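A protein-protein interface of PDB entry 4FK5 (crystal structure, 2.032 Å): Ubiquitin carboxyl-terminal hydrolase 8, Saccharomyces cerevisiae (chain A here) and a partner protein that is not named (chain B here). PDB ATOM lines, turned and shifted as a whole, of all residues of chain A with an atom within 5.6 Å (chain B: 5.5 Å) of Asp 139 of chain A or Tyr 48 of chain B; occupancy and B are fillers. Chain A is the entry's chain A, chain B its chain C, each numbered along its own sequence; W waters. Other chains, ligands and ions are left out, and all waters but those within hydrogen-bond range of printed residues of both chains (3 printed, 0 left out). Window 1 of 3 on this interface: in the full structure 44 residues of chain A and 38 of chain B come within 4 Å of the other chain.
Water W2 lies within hydrogen-bond range of O of Arg 46 of chain B (2.6 Å), NH2 of Arg 138 of chain A (3.1 Å) and N of Tyr 48 of chain B (3.5 Å).
Water W3 lies within hydrogen-bond range of the backbone carbonyl oxygen of Tyr 49 of chain B (2.7 Å), the backbone NH of Ser 454 of chain A (3.0 Å) and the backbone NH of Ile 58 of chain B (3.5 Å).
Water W1 lies within hydrogen-bond range of NH1 of Arg 138 of chain A and O of Arg 46 of chain B.
The side-chain hydroxyl of Ser 454 of chain A is in hydrogen-bond range of the backbone carbonyl oxygen of Tyr 49 of chain B (2.9 Å).
The side-chain carboxylate of Asp 139 of chain A is in hydrogen-bond range of the side-chain hydroxyl of Tyr 48 of chain B (2.5 Å).
NH2 of Arg 46 of chain B touches CE of Met 135 of chain A, 3.2 Å away.
Tyr 48 of chain B touches Arg 138 of chain A.
CD1 of Leu 141 of chain A touches CZ of Tyr 48 of chain B (3.5 Å).
Tyr 48 of chain B touches Phe 445 of chain A.
CG2 of Ile 58 of chain B touches CE1 of Phe 445 of chain A, 3.6 Å away.
OG of Ser 454 of chain A touches CA of Phe 50 of chain B, at 3.3 Å.
Ser 454 of chain A touches Ile 58 of chain B (N to CG2, 3.9 Å).
Hydrophobic or aromatic side chains of chain A that line the printed part of chain B: Met 135, Leu 141 and Phe 445.
Of the 6 printed residues of chain B, 5 touch a printed residue of chain A.
Among the printed residues, 9 pairs touch across the chains.
Among the printed residues, no Asp or Glu carboxylate lies within 4 Å of a Lys or Arg side-chain nitrogen of the other chain.
Printed residues of chain B within 4 Å of Met 135 of chain A: Arg 46.
Printed residues of chain B within 4 Å of Phe 445 of chain A: Tyr 48 and Ile 58.
Printed residues of chain B within 4 Å of Ser 454 of chain A: Tyr 49, Phe 50 and Ile 58.
Of the printed residues of chain A, Tyr 49 of chain B touches Ser 454.
Of the printed residues of chain A, Phe 50 of chain B touches Ser 454 (3.3 Å).
OD2 of Asp 139 of chain A lies within salt-bridge range of NH2 of Arg 138 of chain A.
O of Ile 58 of chain B is in hydrogen-bond range of N of Tyr 49 of chain B (2.9 Å).
The guanidinium group (NH1) of Arg 137 of chain A sits at hydrogen-bond distance from the backbone carbonyl oxygen (O) of Leu 141 of chain A, at 3.1 Å.
The backbone carbonyl oxygen (O) of Met 135 of chain A lies within hydrogen-bond range of the guanidinium group (NH1) of Arg 138 of chain A (2.9 Å).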
ATOM      1  N   MET A 135      11.810 -23.087  -4.890  1.00  0.00           N
ATOM      2  CA  MET A 135      11.451 -22.941  -3.532  1.00  0.00           C
ATOM      3  C   MET A 135      12.610 -23.300  -2.574  1.00  0.00           C
ATOM      4  O   MET A 135      12.874 -22.582  -1.609  1.00  0.00           O
ATOM      5  CB  MET A 135      10.248 -23.806  -3.240  1.00  0.00           C
ATOM      6  CG  MET A 135       9.660 -23.573  -1.883  1.00  0.00           C
ATOM      7  SD  MET A 135       8.261 -24.679  -1.492  1.00  0.00           S
ATOM      8  CE  MET A 135       9.125 -26.147  -0.888  1.00  0.00           C
ATOM      9  N   GLU A 136      13.272 -24.410  -2.841  1.00  0.00           N
ATOM     10  CA  GLU A 136      14.300 -24.920  -1.967  1.00  0.00           C
ATOM     11  C   GLU A 136      15.603 -24.107  -1.997  1.00  0.00           C
ATOM     12  O   GLU A 136      16.398 -24.213  -1.093  1.00  0.00           O
ATOM     13  CB  GLU A 136      14.622 -26.374  -2.354  1.00  0.00           C
ATOM     14  CG  GLU A 136      13.465 -27.356  -2.094  1.00  0.00           C
ATOM     15  CD  GLU A 136      12.449 -27.430  -3.233  1.00  0.00           C
ATOM     16  OE1 GLU A 136      11.472 -28.208  -3.066  1.00  0.00           O
ATOM     17  OE2 GLU A 136      12.601 -26.705  -4.289  1.00  0.00           O
ATOM     18  N   ARG A 137      15.873 -23.409  -3.088  1.00  0.00           N
ATOM     19  CA  ARG A 137      17.198 -22.751  -3.250  1.00  0.00           C
ATOM     20  C   ARG A 137      17.077 -21.222  -3.044  1.00  0.00           C
ATOM     21  O   ARG A 137      18.097 -20.491  -3.007  1.00  0.00           O
ATOM     22  CB  ARG A 137      17.778 -23.031  -4.640  1.00  0.00           C
ATOM     23  CG  ARG A 137      18.055 -24.535  -4.956  1.00  0.00           C
ATOM     24  CD  ARG A 137      19.233 -25.061  -4.189  1.00  0.00           C
ATOM     25  NE  ARG A 137      18.827 -25.787  -2.997  1.00  0.00           N
ATOM     26  CZ  ARG A 137      19.167 -25.472  -1.742  1.00  0.00           C
ATOM     27  NH1 ARG A 137      19.962 -24.407  -1.472  1.00  0.00           N
ATOM     28  NH2 ARG A 137      18.744 -26.250  -0.732  1.00  0.00           N
ATOM     29  N   ARG A 138      15.839 -20.745  -2.919  1.00  0.00           N
ATOM     30  CA  ARG A 138      15.557 -19.312  -2.985  1.00  0.00           C
ATOM     31  C   ARG A 138      16.305 -18.499  -1.910  1.00  0.00           C
ATOM     32  O   ARG A 138      16.680 -17.345  -2.166  1.00  0.00           O
ATOM     33  CB  ARG A 138      14.077 -19.041  -2.872  1.00  0.00           C
ATOM     34  CG  ARG A 138      13.512 -19.242  -1.431  1.00  0.00           C
ATOM     35  CD  ARG A 138      12.017 -19.138  -1.436  1.00  0.00           C
ATOM     36  NE  ARG A 138      11.512 -18.945  -0.083  1.00  0.00           N
ATOM     37  CZ  ARG A 138      11.215 -19.920   0.761  1.00  0.00           C
ATOM     38  NH1 ARG A 138      11.373 -21.184   0.424  1.00  0.00           N
ATOM     39  NH2 ARG A 138      10.817 -19.617   1.981  1.00  0.00           N
ATOM     40  N   ASP A 139      16.574 -19.102  -0.749  1.00  0.00           N
ATOM     41  CA  ASP A 139      17.338 -18.413   0.311  1.00  0.00           C
ATOM     42  C   ASP A 139      18.824 -18.860   0.438  1.00  0.00           C
ATOM     43  O   ASP A 139      19.534 -18.398   1.307  1.00  0.00           O
ATOM     44  CB  ASP A 139      16.636 -18.576   1.644  1.00  0.00           C
ATOM     45  CG  ASP A 139      15.238 -17.892   1.671  1.00  0.00           C
ATOM     46  OD1 ASP A 139      15.088 -16.822   1.051  1.00  0.00           O
ATOM     47  OD2 ASP A 139      14.317 -18.448   2.316  1.00  0.00           O
ATOM     48  N   GLY A 140      19.272 -19.706  -0.469  1.00  0.00           N
ATOM     49  CA  GLY A 140      20.645 -20.127  -0.508  1.00  0.00           C
ATOM     50  C   GLY A 140      21.076 -21.027   0.621  1.00  0.00           C
ATOM     51  O   GLY A 140      22.279 -21.110   0.913  1.00  0.00           O
ATOM     52  N   LEU A 141      20.118 -21.676   1.292  1.00  0.00           N
ATOM     53  CA  LEU A 141      20.413 -22.407   2.506  1.00  0.00           C
ATOM     54  C   LEU A 141      20.875 -23.823   2.168  1.00  0.00           C
ATOM     55  O   LEU A 141      20.144 -24.551   1.624  1.00  0.00           O
ATOM     56  CB  LEU A 141      19.177 -22.503   3.404  1.00  0.00           C
ATOM     57  CG  LEU A 141      18.642 -21.175   3.912  1.00  0.00           C
ATOM     58  CD1 LEU A 141      17.274 -21.342   4.612  1.00  0.00           C
ATOM     59  CD2 LEU A 141      19.665 -20.506   4.843  1.00  0.00           C
ATOM     60  N   HIS A 162      25.910 -15.437   2.593  1.00  0.00           N
ATOM     61  CA  HIS A 162      24.759 -14.723   3.064  1.00  0.00           C
ATOM     62  C   HIS A 162      24.996 -13.204   3.234  1.00  0.00           C
ATOM     63  O   HIS A 162      24.276 -12.577   3.904  1.00  0.00           O
ATOM     64  CB  HIS A 162      24.221 -15.386   4.343  1.00  0.00           C
ATOM     65  CG  HIS A 162      23.605 -16.765   4.065  1.00  0.00           C
ATOM     66  ND1 HIS A 162      22.492 -16.907   3.307  1.00  0.00           N
ATOM     67  CD2 HIS A 162      24.121 -18.055   4.259  1.00  0.00           C
ATOM     68  CE1 HIS A 162      22.241 -18.230   3.099  1.00  0.00           C
ATOM     69  NE2 HIS A 162      23.235 -18.941   3.695  1.00  0.00           N
ATOM     70  N   LEU A 199      24.114 -23.001  -4.544  1.00  0.00           N
ATOM     71  CA  LEU A 199      23.248 -22.792  -3.378  1.00  0.00           C
ATOM     72  C   LEU A 199      21.946 -22.072  -3.751  1.00  0.00           C
ATOM     73  O   LEU A 199      20.901 -22.304  -3.140  1.00  0.00           O
ATOM     74  CB  LEU A 199      24.013 -22.039  -2.274  1.00  0.00           C
ATOM     75  CG  LEU A 199      24.705 -22.990  -1.257  1.00  0.00           C
ATOM     76  CD1 LEU A 199      25.580 -23.985  -1.964  1.00  0.00           C
ATOM     77  CD2 LEU A 199      25.522 -22.240  -0.190  1.00  0.00           C
ATOM     78  N   TYR A 200      22.025 -21.206  -4.761  1.00  0.00           N
ATOM     79  CA  TYR A 200      20.910 -20.349  -5.150  1.00  0.00           C
ATOM     80  C   TYR A 200      20.272 -20.788  -6.503  1.00  0.00           C
ATOM     81  O   TYR A 200      19.090 -20.533  -6.773  1.00  0.00           O
ATOM     82  CB  TYR A 200      21.390 -18.920  -5.228  1.00  0.00           C
ATOM     83  CG  TYR A 200      21.597 -18.257  -3.897  1.00  0.00           C
ATOM     84  CD1 TYR A 200      20.537 -17.643  -3.229  1.00  0.00           C
ATOM     85  CD2 TYR A 200      22.873 -18.135  -3.355  1.00  0.00           C
ATOM     86  CE1 TYR A 200      20.747 -16.955  -1.997  1.00  0.00           C
ATOM     87  CE2 TYR A 200      23.082 -17.488  -2.174  1.00  0.00           C
ATOM     88  CZ  TYR A 200      22.018 -16.897  -1.490  1.00  0.00           C
ATOM     89  OH  TYR A 200      22.268 -16.261  -0.258  1.00  0.00           O
ATOM     90  N   ILE A 439      18.805 -13.776   7.666  1.00  0.00           N
ATOM     91  CA  ILE A 439      18.342 -13.436   6.337  1.00  0.00           C
ATOM     92  C   ILE A 439      17.101 -12.544   6.427  1.00  0.00           C
ATOM     93  O   ILE A 439      16.560 -12.296   7.518  1.00  0.00           O
ATOM     94  CB  ILE A 439      18.049 -14.684   5.468  1.00  0.00           C
ATOM     95  CG1 ILE A 439      16.811 -15.437   5.947  1.00  0.00           C
ATOM     96  CG2 ILE A 439      19.274 -15.595   5.405  1.00  0.00           C
ATOM     97  CD1 ILE A 439      16.452 -16.591   5.013  1.00  0.00           C
ATOM     98  N   PHE A 445      19.592 -18.565  11.012  1.00  0.00           N
ATOM     99  CA  PHE A 445      19.904 -19.942  10.756  1.00  0.00           C
ATOM    100  C   PHE A 445      21.257 -20.297  11.314  1.00  0.00           C
ATOM    101  O   PHE A 445      22.188 -19.440  11.329  1.00  0.00           O
ATOM    102  CB  PHE A 445      19.818 -20.205   9.239  1.00  0.00           C
ATOM    103  CG  PHE A 445      18.448 -20.122   8.719  1.00  0.00           C
ATOM    104  CD1 PHE A 445      17.596 -21.210   8.795  1.00  0.00           C
ATOM    105  CD2 PHE A 445      17.947 -18.906   8.226  1.00  0.00           C
ATOM    106  CE1 PHE A 445      16.300 -21.116   8.390  1.00  0.00           C
ATOM    107  CE2 PHE A 445      16.644 -18.804   7.856  1.00  0.00           C
ATOM    108  CZ  PHE A 445      15.817 -19.935   7.905  1.00  0.00           C
ATOM    109  N   SER A 454      16.915 -23.717  12.052  1.00  0.00           N
ATOM    110  CA  SER A 454      16.400 -22.424  12.484  1.00  0.00           C
ATOM    111  C   SER A 454      16.609 -22.276  13.965  1.00  0.00           C
ATOM    112  O   SER A 454      16.660 -23.261  14.698  1.00  0.00           O
ATOM    113  CB  SER A 454      14.932 -22.254  12.107  1.00  0.00           C
ATOM    114  OG  SER A 454      14.200 -23.285  12.630  1.00  0.00           O
ATOM    115  N   ARG B  46       6.137 -24.405   2.242  1.00  0.00           N
ATOM    116  CA  ARG B  46       6.223 -24.787   3.674  1.00  0.00           C
ATOM    117  C   ARG B  46       7.199 -23.892   4.461  1.00  0.00           C
ATOM    118  O   ARG B  46       8.173 -23.468   3.948  1.00  0.00           O
ATOM    119  CB  ARG B  46       6.676 -26.231   3.794  1.00  0.00           C
ATOM    120  CG  ARG B  46       5.548 -27.238   3.704  1.00  0.00           C
ATOM    121  CD  ARG B  46       6.082 -28.644   3.492  1.00  0.00           C
ATOM    122  NE  ARG B  46       6.843 -28.752   2.227  1.00  0.00           N
ATOM    123  CZ  ARG B  46       8.178 -28.726   2.128  1.00  0.00           C
ATOM    124  NH1 ARG B  46       8.937 -28.606   3.217  1.00  0.00           N
ATOM    125  NH2 ARG B  46       8.758 -28.816   0.929  1.00  0.00           N
ATOM    126  N   SER B  47       6.871 -23.592   5.699  1.00  0.00           N
ATOM    127  CA  SER B  47       7.796 -23.004   6.634  1.00  0.00           C
ATOM    128  C   SER B  47       9.070 -23.856   6.797  1.00  0.00           C
ATOM    129  O   SER B  47       9.017 -25.059   6.736  1.00  0.00           O
ATOM    130  CB  SER B  47       7.119 -22.896   7.992  1.00  0.00           C
ATOM    131  OG  SER B  47       6.688 -21.573   8.241  1.00  0.00           O
ATOM    132  N   TYR B  48      10.210 -23.229   7.056  1.00  0.00           N
ATOM    133  CA  TYR B  48      11.348 -23.988   7.499  1.00  0.00           C
ATOM    134  C   TYR B  48      10.996 -24.588   8.838  1.00  0.00           C
ATOM    135  O   TYR B  48      10.386 -23.939   9.665  1.00  0.00           O
ATOM    136  CB  TYR B  48      12.591 -23.096   7.602  1.00  0.00           C
ATOM    137  CG  TYR B  48      13.058 -22.527   6.252  1.00  0.00           C
ATOM    138  CD1 TYR B  48      13.359 -23.380   5.159  1.00  0.00           C
ATOM    139  CD2 TYR B  48      13.090 -21.181   6.041  1.00  0.00           C
ATOM    140  CE1 TYR B  48      13.791 -22.873   3.947  1.00  0.00           C
ATOM    141  CE2 TYR B  48      13.518 -20.642   4.840  1.00  0.00           C
ATOM    142  CZ  TYR B  48      13.884 -21.482   3.788  1.00  0.00           C
ATOM    143  OH  TYR B  48      14.265 -20.902   2.591  1.00  0.00           O
ATOM    144  N   TYR B  49      11.349 -25.838   9.039  1.00  0.00           N
ATOM    145  CA  TYR B  49      11.125 -26.503  10.304  1.00  0.00           C
ATOM    146  C   TYR B  49      11.922 -25.844  11.474  1.00  0.00           C
ATOM    147  O   TYR B  49      13.146 -25.647  11.375  1.00  0.00           O
ATOM    148  CB  TYR B  49      11.492 -27.991  10.172  1.00  0.00           C
ATOM    149  CG  TYR B  49      10.968 -28.876  11.292  1.00  0.00           C
ATOM    150  CD1 TYR B  49      11.712 -29.057  12.475  1.00  0.00           C
ATOM    151  CD2 TYR B  49       9.772 -29.548  11.169  1.00  0.00           C
ATOM    152  CE1 TYR B  49      11.248 -29.838  13.506  1.00  0.00           C
ATOM    153  CE2 TYR B  49       9.290 -30.373  12.216  1.00  0.00           C
ATOM    154  CZ  TYR B  49      10.028 -30.510  13.374  1.00  0.00           C
ATOM    155  OH  TYR B  49       9.578 -31.319  14.426  1.00  0.00           O
ATOM    156  N   PHE B  50      11.212 -25.594  12.595  1.00  0.00           N
ATOM    157  CA  PHE B  50      11.825 -25.188  13.851  1.00  0.00           C
ATOM    158  C   PHE B  50      11.683 -26.265  14.921  1.00  0.00           C
ATOM    159  O   PHE B  50      10.603 -26.758  15.159  1.00  0.00           O
ATOM    160  CB  PHE B  50      11.212 -23.875  14.373  1.00  0.00           C
ATOM    161  CG  PHE B  50      11.747 -23.463  15.719  1.00  0.00           C
ATOM    162  CD1 PHE B  50      13.053 -23.021  15.852  1.00  0.00           C
ATOM    163  CD2 PHE B  50      10.953 -23.567  16.871  1.00  0.00           C
ATOM    164  CE1 PHE B  50      13.574 -22.676  17.100  1.00  0.00           C
ATOM    165  CE2 PHE B  50      11.465 -23.229  18.128  1.00  0.00           C
ATOM    166  CZ  PHE B  50      12.775 -22.769  18.240  1.00  0.00           C
ATOM    167  N   ILE B  58      16.201 -27.803   8.986  1.00  0.00           N
ATOM    168  CA  ILE B  58      15.139 -27.018   8.416  1.00  0.00           C
ATOM    169  C   ILE B  58      14.122 -27.849   7.602  1.00  0.00           C
ATOM    170  O   ILE B  58      13.020 -27.349   7.248  1.00  0.00           O
ATOM    171  CB  ILE B  58      15.653 -25.856   7.500  1.00  0.00           C
ATOM    172  CG1 ILE B  58      16.563 -26.381   6.380  1.00  0.00           C
ATOM    173  CG2 ILE B  58      16.318 -24.748   8.329  1.00  0.00           C
ATOM    174  CD1 ILE B  58      17.093 -25.263   5.476  1.00  0.00           C
HETATM  175  O   HOH W   1      10.738 -23.792   1.849  1.00  0.00           O
HETATM  176  O   HOH W   2      10.392 -22.156   3.754  1.00  0.00           O
HETATM  177  O   HOH W   3      15.642 -26.445  12.159  1.00  0.00           O
